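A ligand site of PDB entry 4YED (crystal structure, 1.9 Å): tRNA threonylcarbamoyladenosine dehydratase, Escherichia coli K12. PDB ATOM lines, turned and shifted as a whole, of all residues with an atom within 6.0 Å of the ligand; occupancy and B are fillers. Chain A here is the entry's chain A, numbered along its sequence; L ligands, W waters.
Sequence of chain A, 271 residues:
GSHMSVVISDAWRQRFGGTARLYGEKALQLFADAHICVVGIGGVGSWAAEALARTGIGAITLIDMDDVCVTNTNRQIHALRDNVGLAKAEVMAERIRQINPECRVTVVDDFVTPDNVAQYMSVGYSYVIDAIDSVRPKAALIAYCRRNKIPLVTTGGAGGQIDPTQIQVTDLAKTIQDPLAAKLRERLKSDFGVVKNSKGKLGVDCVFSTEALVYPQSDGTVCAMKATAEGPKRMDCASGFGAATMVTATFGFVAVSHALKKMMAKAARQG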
ATOM      1  N   VAL A  39       4.797 -31.669   2.543  1.00  0.00           N
ATOM      2  CA  VAL A  39       4.870 -30.520   3.425  1.00  0.00           C
ATOM      3  C   VAL A  39       4.229 -29.338   2.770  1.00  0.00           C
ATOM      4  O   VAL A  39       4.675 -28.874   1.754  1.00  0.00           O
ATOM      5  CB  VAL A  39       6.324 -30.231   3.898  1.00  0.00           C
ATOM      6  CG1 VAL A  39       6.329 -29.191   4.980  1.00  0.00           C
ATOM      7  CG2 VAL A  39       6.980 -31.487   4.369  1.00  0.00           C
ATOM      8  N   GLY A  40       3.122 -28.897   3.374  1.00  0.00           N
ATOM      9  CA  GLY A  40       2.319 -27.873   2.837  1.00  0.00           C
ATOM     10  C   GLY A  40       1.175 -28.400   1.998  1.00  0.00           C
ATOM     11  O   GLY A  40       1.374 -28.893   0.867  1.00  0.00           O
ATOM     12  N   ILE A  41      -0.039 -28.319   2.550  1.00  0.00           N
ATOM     13  CA  ILE A  41      -1.228 -28.898   1.953  1.00  0.00           C
ATOM     14  C   ILE A  41      -2.089 -27.807   1.296  1.00  0.00           C
ATOM     15  O   ILE A  41      -3.333 -27.694   1.551  1.00  0.00           O
ATOM     16  CB  ILE A  41      -2.010 -29.780   2.985  1.00  0.00           C
ATOM     17  CG1 ILE A  41      -1.096 -30.706   3.767  1.00  0.00           C
ATOM     18  CG2 ILE A  41      -3.061 -30.632   2.267  1.00  0.00           C
ATOM     19  CD1 ILE A  41      -0.229 -31.661   2.909  1.00  0.00           C
ATOM     20  N   GLY A  42      -1.464 -27.043   0.410  1.00  0.00           N
ATOM     21  CA  GLY A  42      -2.066 -25.846  -0.196  1.00  0.00           C
ATOM     22  C   GLY A  42      -2.342 -26.014  -1.661  1.00  0.00           C
ATOM     23  O   GLY A  42      -2.672 -27.104  -2.142  1.00  0.00           O
ATOM     24  N   GLY A  43      -2.090 -24.966  -2.430  1.00  0.00           N
ATOM     25  CA  GLY A  43      -2.411 -24.945  -3.839  1.00  0.00           C
ATOM     26  C   GLY A  43      -1.684 -26.052  -4.615  1.00  0.00           C
ATOM     27  O   GLY A  43      -2.197 -26.536  -5.649  1.00  0.00           O
ATOM     28  N   VAL A  44      -0.438 -26.330  -4.218  1.00  0.00           N
ATOM     29  CA  VAL A  44       0.332 -27.401  -4.818  1.00  0.00           C
ATOM     30  C   VAL A  44       0.217 -28.700  -4.050  1.00  0.00           C
ATOM     31  O   VAL A  44      -0.103 -29.762  -4.610  1.00  0.00           O
ATOM     32  CB  VAL A  44       1.758 -26.992  -4.918  1.00  0.00           C
ATOM     33  CG1 VAL A  44       2.614 -28.115  -5.498  1.00  0.00           C
ATOM     34  CG2 VAL A  44       1.887 -25.828  -5.890  1.00  0.00           C
ATOM     35  N   ILE A  63       2.026 -32.523   6.468  1.00  0.00           N
ATOM     36  CA  ILE A  63       2.494 -31.578   7.436  1.00  0.00           C
ATOM     37  C   ILE A  63       2.032 -30.166   7.059  1.00  0.00           C
ATOM     38  O   ILE A  63       2.466 -29.589   6.085  1.00  0.00           O
ATOM     39  CB  ILE A  63       4.048 -31.628   7.677  1.00  0.00           C
ATOM     40  CG1 ILE A  63       4.573 -33.021   7.861  1.00  0.00           C
ATOM     41  CG2 ILE A  63       4.437 -30.762   8.887  1.00  0.00           C
ATOM     42  CD1 ILE A  63       6.080 -33.085   8.004  1.00  0.00           C
ATOM     43  N   ASP A  64       1.154 -29.603   7.905  1.00  0.00           N
ATOM     44  CA  ASP A  64       0.662 -28.225   7.728  1.00  0.00           C
ATOM     45  C   ASP A  64      -0.130 -27.861   8.991  1.00  0.00           C
ATOM     46  O   ASP A  64      -0.699 -28.706   9.651  1.00  0.00           O
ATOM     47  CB  ASP A  64      -0.256 -28.151   6.478  1.00  0.00           C
ATOM     48  CG  ASP A  64      -0.471 -26.744   5.920  1.00  0.00           C
ATOM     49  OD1 ASP A  64      -0.382 -25.719   6.668  1.00  0.00           O
ATOM     50  OD2 ASP A  64      -0.752 -26.656   4.694  1.00  0.00           O
ATOM     51  N   MET A  65      -0.134 -26.586   9.350  1.00  0.00           N
ATOM     52  CA  MET A  65      -0.931 -26.142  10.514  1.00  0.00           C
ATOM     53  C   MET A  65      -2.080 -25.261  10.112  1.00  0.00           C
ATOM     54  O   MET A  65      -2.943 -24.943  10.938  1.00  0.00           O
ATOM     55  CB  MET A  65       0.025 -25.386  11.475  1.00  0.00           C
ATOM     56  CG  MET A  65      -0.308 -25.750  12.905  1.00  0.00           C
ATOM     57  SD  MET A  65       0.652 -24.598  14.244  1.00  0.00           S
ATOM     58  CE  MET A  65       1.800 -23.475  13.070  1.00  0.00           C
ATOM     59  N   ASP A  66      -2.186 -24.885   8.845  1.00  0.00           N
ATOM     60  CA  ASP A  66      -3.258 -24.015   8.448  1.00  0.00           C
ATOM     61  C   ASP A  66      -4.630 -24.635   8.336  1.00  0.00           C
ATOM     62  O   ASP A  66      -4.818 -25.831   8.227  1.00  0.00           O
ATOM     63  CB  ASP A  66      -2.932 -23.304   7.171  1.00  0.00           C
ATOM     64  CG  ASP A  66      -2.517 -21.926   7.415  1.00  0.00           C
ATOM     65  OD1 ASP A  66      -3.417 -21.092   7.786  1.00  0.00           O
ATOM     66  OD2 ASP A  66      -1.297 -21.711   7.286  1.00  0.00           O
ATOM     67  N   ASN A  72      -9.258 -20.246  -0.396  1.00  0.00           N
ATOM     68  CA  ASN A  72      -8.499 -21.345  -1.017  1.00  0.00           C
ATOM     69  C   ASN A  72      -9.268 -21.958  -2.208  1.00  0.00           C
ATOM     70  O   ASN A  72      -8.689 -22.751  -2.906  1.00  0.00           O
ATOM     71  CB  ASN A  72      -8.230 -22.463  -0.045  1.00  0.00           C
ATOM     72  CG  ASN A  72      -7.480 -22.050   1.211  1.00  0.00           C
ATOM     73  OD1 ASN A  72      -7.626 -22.716   2.223  1.00  0.00           O
ATOM     74  ND2 ASN A  72      -6.716 -20.954   1.162  1.00  0.00           N
ATOM     75  N   ARG A  75      -8.023 -22.982  -5.894  1.00  0.00           N
ATOM     76  CA  ARG A  75      -6.810 -23.736  -6.144  1.00  0.00           C
ATOM     77  C   ARG A  75      -6.497 -24.901  -5.208  1.00  0.00           C
ATOM     78  O   ARG A  75      -5.451 -25.521  -5.385  1.00  0.00           O
ATOM     79  CB  ARG A  75      -5.649 -22.766  -6.172  1.00  0.00           C
ATOM     80  CG  ARG A  75      -5.204 -22.299  -4.769  1.00  0.00           C
ATOM     81  CD  ARG A  75      -4.432 -20.992  -4.827  1.00  0.00           C
ATOM     82  NE  ARG A  75      -3.926 -20.534  -3.531  1.00  0.00           N
ATOM     83  CZ  ARG A  75      -4.608 -19.897  -2.604  1.00  0.00           C
ATOM     84  NH1 ARG A  75      -5.896 -19.590  -2.753  1.00  0.00           N
ATOM     85  NH2 ARG A  75      -3.988 -19.527  -1.493  1.00  0.00           N
ATOM     86  N   GLN A  76      -7.357 -25.248  -4.242  1.00  0.00           N
ATOM     87  CA  GLN A  76      -7.018 -26.325  -3.293  1.00  0.00           C
ATOM     88  C   GLN A  76      -8.136 -27.352  -3.216  1.00  0.00           C
ATOM     89  O   GLN A  76      -9.367 -27.030  -3.090  1.00  0.00           O
ATOM     90  CB  GLN A  76      -6.679 -25.753  -1.853  1.00  0.00           C
ATOM     91  CG  GLN A  76      -5.649 -24.643  -1.929  1.00  0.00           C
ATOM     92  CD  GLN A  76      -5.178 -24.029  -0.605  1.00  0.00           C
ATOM     93  OE1 GLN A  76      -5.245 -24.595   0.425  1.00  0.00           O
ATOM     94  NE2 GLN A  76      -4.572 -22.882  -0.716  1.00  0.00           N
ATOM     95  N   LYS A  88      -6.553 -28.064   7.397  1.00  0.00           N
ATOM     96  CA  LYS A  88      -6.290 -28.628   6.032  1.00  0.00           C
ATOM     97  C   LYS A  88      -5.775 -30.021   6.039  1.00  0.00           C
ATOM     98  O   LYS A  88      -6.270 -30.879   5.283  1.00  0.00           O
ATOM     99  CB  LYS A  88      -5.253 -27.798   5.279  1.00  0.00           C
ATOM    100  CG  LYS A  88      -5.697 -26.500   4.811  1.00  0.00           C
ATOM    101  CD  LYS A  88      -4.570 -25.753   4.141  1.00  0.00           C
ATOM    102  CE  LYS A  88      -5.055 -24.398   3.737  1.00  0.00           C
ATOM    103  NZ  LYS A  88      -4.032 -23.668   2.943  1.00  0.00           N
ATOM    104  N   ASP A 110       1.632 -28.900  12.284  1.00  0.00           N
ATOM    105  CA  ASP A 110       2.755 -27.991  12.604  1.00  0.00           C
ATOM    106  C   ASP A 110       3.350 -27.449  11.330  1.00  0.00           C
ATOM    107  O   ASP A 110       2.992 -27.895  10.244  1.00  0.00           O
ATOM    108  CB  ASP A 110       3.824 -28.726  13.410  1.00  0.00           C
ATOM    109  CG  ASP A 110       4.680 -27.805  14.336  1.00  0.00           C
ATOM    110  OD1 ASP A 110       4.581 -26.551  14.286  1.00  0.00           O
ATOM    111  OD2 ASP A 110       5.513 -28.387  15.089  1.00  0.00           O
ATOM    112  N   PHE A 111       4.197 -26.444  11.442  1.00  0.00           N
ATOM    113  CA  PHE A 111       5.052 -25.957  10.341  1.00  0.00           C
ATOM    114  C   PHE A 111       6.452 -26.450  10.581  1.00  0.00           C
ATOM    115  O   PHE A 111       6.839 -26.684  11.721  1.00  0.00           O
ATOM    116  CB  PHE A 111       5.086 -24.398  10.223  1.00  0.00           C
ATOM    117  CG  PHE A 111       3.754 -23.764   9.847  1.00  0.00           C
ATOM    118  CD1 PHE A 111       2.928 -24.296   8.826  1.00  0.00           C
ATOM    119  CD2 PHE A 111       3.287 -22.623  10.533  1.00  0.00           C
ATOM    120  CE1 PHE A 111       1.696 -23.716   8.512  1.00  0.00           C
ATOM    121  CE2 PHE A 111       2.041 -22.041  10.219  1.00  0.00           C
ATOM    122  CZ  PHE A 111       1.256 -22.589   9.198  1.00  0.00           C
ATOM    123  N   VAL A 112       7.205 -26.654   9.508  1.00  0.00           N
ATOM    124  CA  VAL A 112       8.585 -27.065   9.592  1.00  0.00           C
ATOM    125  C   VAL A 112       9.440 -25.877   9.978  1.00  0.00           C
ATOM    126  O   VAL A 112       9.200 -24.758   9.494  1.00  0.00           O
ATOM    127  CB  VAL A 112       9.017 -27.703   8.259  1.00  0.00           C
ATOM    128  CG1 VAL A 112      10.539 -27.782   8.169  1.00  0.00           C
ATOM    129  CG2 VAL A 112       8.377 -29.069   8.132  1.00  0.00           C
ATOM    130  N   THR A 113      10.392 -26.080  10.889  1.00  0.00           N
ATOM    131  CA  THR A 113      11.371 -25.020  11.232  1.00  0.00           C
ATOM    132  C   THR A 113      12.761 -25.624  11.381  1.00  0.00           C
ATOM    133  O   THR A 113      12.926 -26.877  11.464  1.00  0.00           O
ATOM    134  CB  THR A 113      11.060 -24.348  12.633  1.00  0.00           C
ATOM    135  OG1 THR A 113      11.386 -25.271  13.673  1.00  0.00           O
ATOM    136  CG2 THR A 113       9.627 -23.928  12.748  1.00  0.00           C
ATOM    137  N   ALA A 131       6.069 -28.554  -0.727  1.00  0.00           N
ATOM    138  CA  ALA A 131       5.080 -27.626  -1.303  1.00  0.00           C
ATOM    139  C   ALA A 131       4.827 -26.472  -0.359  1.00  0.00           C
ATOM    140  O   ALA A 131       3.704 -25.984  -0.250  1.00  0.00           O
ATOM    141  CB  ALA A 131       3.794 -28.381  -1.564  1.00  0.00           C
ATOM    142  N   ILE A 132       5.869 -26.043   0.355  1.00  0.00           N
ATOM    143  CA  ILE A 132       5.767 -24.930   1.268  1.00  0.00           C
ATOM    144  C   ILE A 132       5.830 -23.594   0.501  1.00  0.00           C
ATOM    145  O   ILE A 132       6.677 -23.405  -0.371  1.00  0.00           O
ATOM    146  CB  ILE A 132       6.965 -24.904   2.258  1.00  0.00           C
ATOM    147  CG1 ILE A 132       6.929 -26.111   3.172  1.00  0.00           C
ATOM    148  CG2 ILE A 132       6.901 -23.655   3.106  1.00  0.00           C
ATOM    149  CD1 ILE A 132       8.207 -26.259   3.985  1.00  0.00           C
ATOM    150  N   ASP A 133       4.982 -22.646   0.877  1.00  0.00           N
ATOM    151  CA  ASP A 133       5.014 -21.344   0.196  1.00  0.00           C
ATOM    152  C   ASP A 133       6.023 -20.367   0.828  1.00  0.00           C
ATOM    153  O   ASP A 133       6.535 -19.566   0.106  1.00  0.00           O
ATOM    154  CB  ASP A 133       3.591 -20.726   0.083  1.00  0.00           C
ATOM    155  CG  ASP A 133       3.085 -20.209   1.404  1.00  0.00           C
ATOM    156  OD1 ASP A 133       3.589 -20.672   2.466  1.00  0.00           O
ATOM    157  OD2 ASP A 133       2.184 -19.339   1.393  1.00  0.00           O
ATOM    158  N   SER A 134       6.286 -20.431   2.132  1.00  0.00           N
ATOM    159  CA  SER A 134       7.198 -19.439   2.781  1.00  0.00           C
ATOM    160  C   SER A 134       8.620 -19.818   2.609  1.00  0.00           C
ATOM    161  O   SER A 134       8.972 -20.975   2.859  1.00  0.00           O
ATOM    162  CB  SER A 134       7.011 -19.379   4.290  1.00  0.00           C
ATOM    163  OG  SER A 134       5.675 -19.485   4.655  1.00  0.00           O
ATOM    164  N   PRO A 137      10.911 -21.513   6.151  1.00  0.00           N
ATOM    165  CA  PRO A 137      10.777 -22.935   6.418  1.00  0.00           C
ATOM    166  C   PRO A 137      11.136 -23.804   5.216  1.00  0.00           C
ATOM    167  O   PRO A 137      11.696 -24.888   5.376  1.00  0.00           O
ATOM    168  CB  PRO A 137       9.312 -23.084   6.736  1.00  0.00           C
ATOM    169  CG  PRO A 137       8.627 -21.875   6.188  1.00  0.00           C
ATOM    170  CD  PRO A 137       9.625 -20.800   6.198  1.00  0.00           C
ATOM    171  N   LYS A 138      10.773 -23.341   4.024  1.00  0.00           N
ATOM    172  CA  LYS A 138      11.162 -23.992   2.791  1.00  0.00           C
ATOM    173  C   LYS A 138      12.679 -24.211   2.715  1.00  0.00           C
ATOM    174  O   LYS A 138      13.136 -25.316   2.446  1.00  0.00           O
ATOM    175  CB  LYS A 138      10.644 -23.195   1.571  1.00  0.00           C
ATOM    176  CG  LYS A 138      10.755 -23.880   0.230  1.00  0.00           C
ATOM    177  CD  LYS A 138      10.060 -23.037  -0.845  1.00  0.00           C
ATOM    178  CE  LYS A 138       9.744 -23.773  -2.129  1.00  0.00           C
ATOM    179  NZ  LYS A 138       8.644 -24.782  -1.996  1.00  0.00           N
HETATM  180  P1  LIG L   1      -0.786 -21.951  -0.940  1.00  0.00           P
HETATM  181  O1  LIG L   1      -1.519 -21.023   0.064  1.00  0.00           O
HETATM  182  O2  LIG L   1      -1.678 -22.384  -2.066  1.00  0.00           O
HETATM  183  O3  LIG L   1       0.566 -21.455  -1.442  1.00  0.00           O
HETATM  184  O4  LIG L   1      -0.327 -23.196  -0.020  1.00  0.00           O
HETATM  185  C1  LIG L   1       0.783 -23.068   0.871  1.00  0.00           C
HETATM  186  C2  LIG L   1       0.616 -24.013   2.041  1.00  0.00           C
HETATM  187  O5  LIG L   1       1.910 -24.185   2.662  1.00  0.00           O
HETATM  188  C3  LIG L   1      -0.374 -23.513   3.123  1.00  0.00           C
HETATM  189  O6  LIG L   1      -1.372 -24.483   3.516  1.00  0.00           O
HETATM  190  C4  LIG L   1       0.524 -23.201   4.328  1.00  0.00           C
HETATM  191  O7  LIG L   1      -0.181 -23.243   5.607  1.00  0.00           O
HETATM  192  C5  LIG L   1       1.664 -24.228   4.089  1.00  0.00           C
HETATM  193  N1  LIG L   1       2.911 -23.969   4.814  1.00  0.00           N
HETATM  194  C6  LIG L   1       3.519 -22.729   4.886  1.00  0.00           C
HETATM  195  N2  LIG L   1       4.658 -22.788   5.637  1.00  0.00           N
HETATM  196  C7  LIG L   1       4.755 -24.059   6.061  1.00  0.00           C
HETATM  197  C8  LIG L   1       5.761 -24.785   6.848  1.00  0.00           C
HETATM  198  N3  LIG L   1       6.778 -24.042   7.326  1.00  0.00           N
HETATM  199  N4  LIG L   1       5.625 -26.107   7.072  1.00  0.00           N
HETATM  200  C9  LIG L   1       4.500 -26.805   6.580  1.00  0.00           C
HETATM  201  N5  LIG L   1       3.537 -26.236   5.816  1.00  0.00           N
HETATM  202  C10 LIG L   1       3.619 -24.877   5.508  1.00  0.00           C
HETATM  203  O   HOH W   1       1.107 -24.207  -2.748  1.00  0.00           O
HETATM  204  O   HOH W   2      -1.040 -21.467  -4.659  1.00  0.00           O
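The side-chain carboxylate (OD2) of Asp 66 sits at hydrogen-bond distance from an oxygen (O7) of the ligand (2.5 Å). An oxygen (O6) of the ligand lies within hydrogen-bond range of the side-chain carboxylate (OD2) of Asp 64 (2.5 Å). An oxygen (O2) of the ligand lies within hydrogen-bond range of the backbone NH (N) of Gly 43, 2.6 Å away. An oxygen (O6) of the ligand sits at hydrogen-bond distance from the side-chain amino group of Lys 88 (2.8 Å). N4 of the ligand sits at hydrogen-bond distance from N of Val 112 (3.0 Å). O of Val 112 lies within hydrogen-bond range of N3 of the ligand (3.3 Å). The side-chain amide nitrogen of Gln 76 is in hydrogen-bond range of an oxygen (O2) of the ligand (3.2 Å). The guanidinium group (NE) of Arg 75 is in salt-bridge range of an oxygen (O2) of the ligand (3.3 Å).
The backbone NH of Asp 66 is in hydrogen-bond range of the side-chain carboxylate of Asp 64 (2.9 Å). The backbone NH (N) of Asp 64 lies close to the backbone carbonyl oxygen (O) of Asp 110, 3.4 Å away. The side-chain amino group (NZ) of Lys 88 sits at hydrogen-bond distance from the side-chain amide oxygen (OE1) of Gln 76 (2.9 Å). OD1 of Asp 133 lies within hydrogen-bond range of OG of Ser 134, at 3.2 Å. The guanidinium group (NH2) of Arg 75 sits close to the side-chain amide nitrogen (NE2) of Gln 76, 3.5 Å away. NE2 of Gln 76 lies close to ND2 of Asn 72 (3.4 Å). The backbone carbonyl oxygen of Val 39 lies within hydrogen-bond range of the backbone NH of Ile 132, 3.4 Å away. The backbone carbonyl oxygen of Ile 132 is in hydrogen-bond range of the side-chain amino group of Lys 138.
Val 39 touches the ligand (CG1 to C9, 3.4 Å). CA of Gly 40 touches N5 of the ligand, at 3.6 Å. Gly 42 touches the ligand. Ile 63 touches the ligand. Phe 111 touches the ligand (CA to N4, 3.3 Å). O of Ala 131 touches O5 of the ligand (3.9 Å). Ile 132 touches the ligand. OD1 of Asp 133 touches C6 of the ligand, 3.2 Å away. Ser 134 touches the ligand. Pro 137 touches the ligand. Hydrophobic or aromatic side chains that line the ligand: Val 39, Phe 111, Val 112, Ile 132 and Pro 137. Within 4 Å of the ligand: Val 39, Gly 40, Gly 42, Gly 43, Ile 63, Asp 64, Asp 66, Arg 75, Gln 76, Lys 88, Phe 111, Val 112, Ala 131, Ile 132, Asp 133, Ser 134 and Pro 137.
Water W2 bridges O2 of the ligand (2.8 Å) and NE of Arg 75 (3.2 Å). Water W1 lies within hydrogen-bond range of N of Val 44, O3 of the ligand and N of Gly 43.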
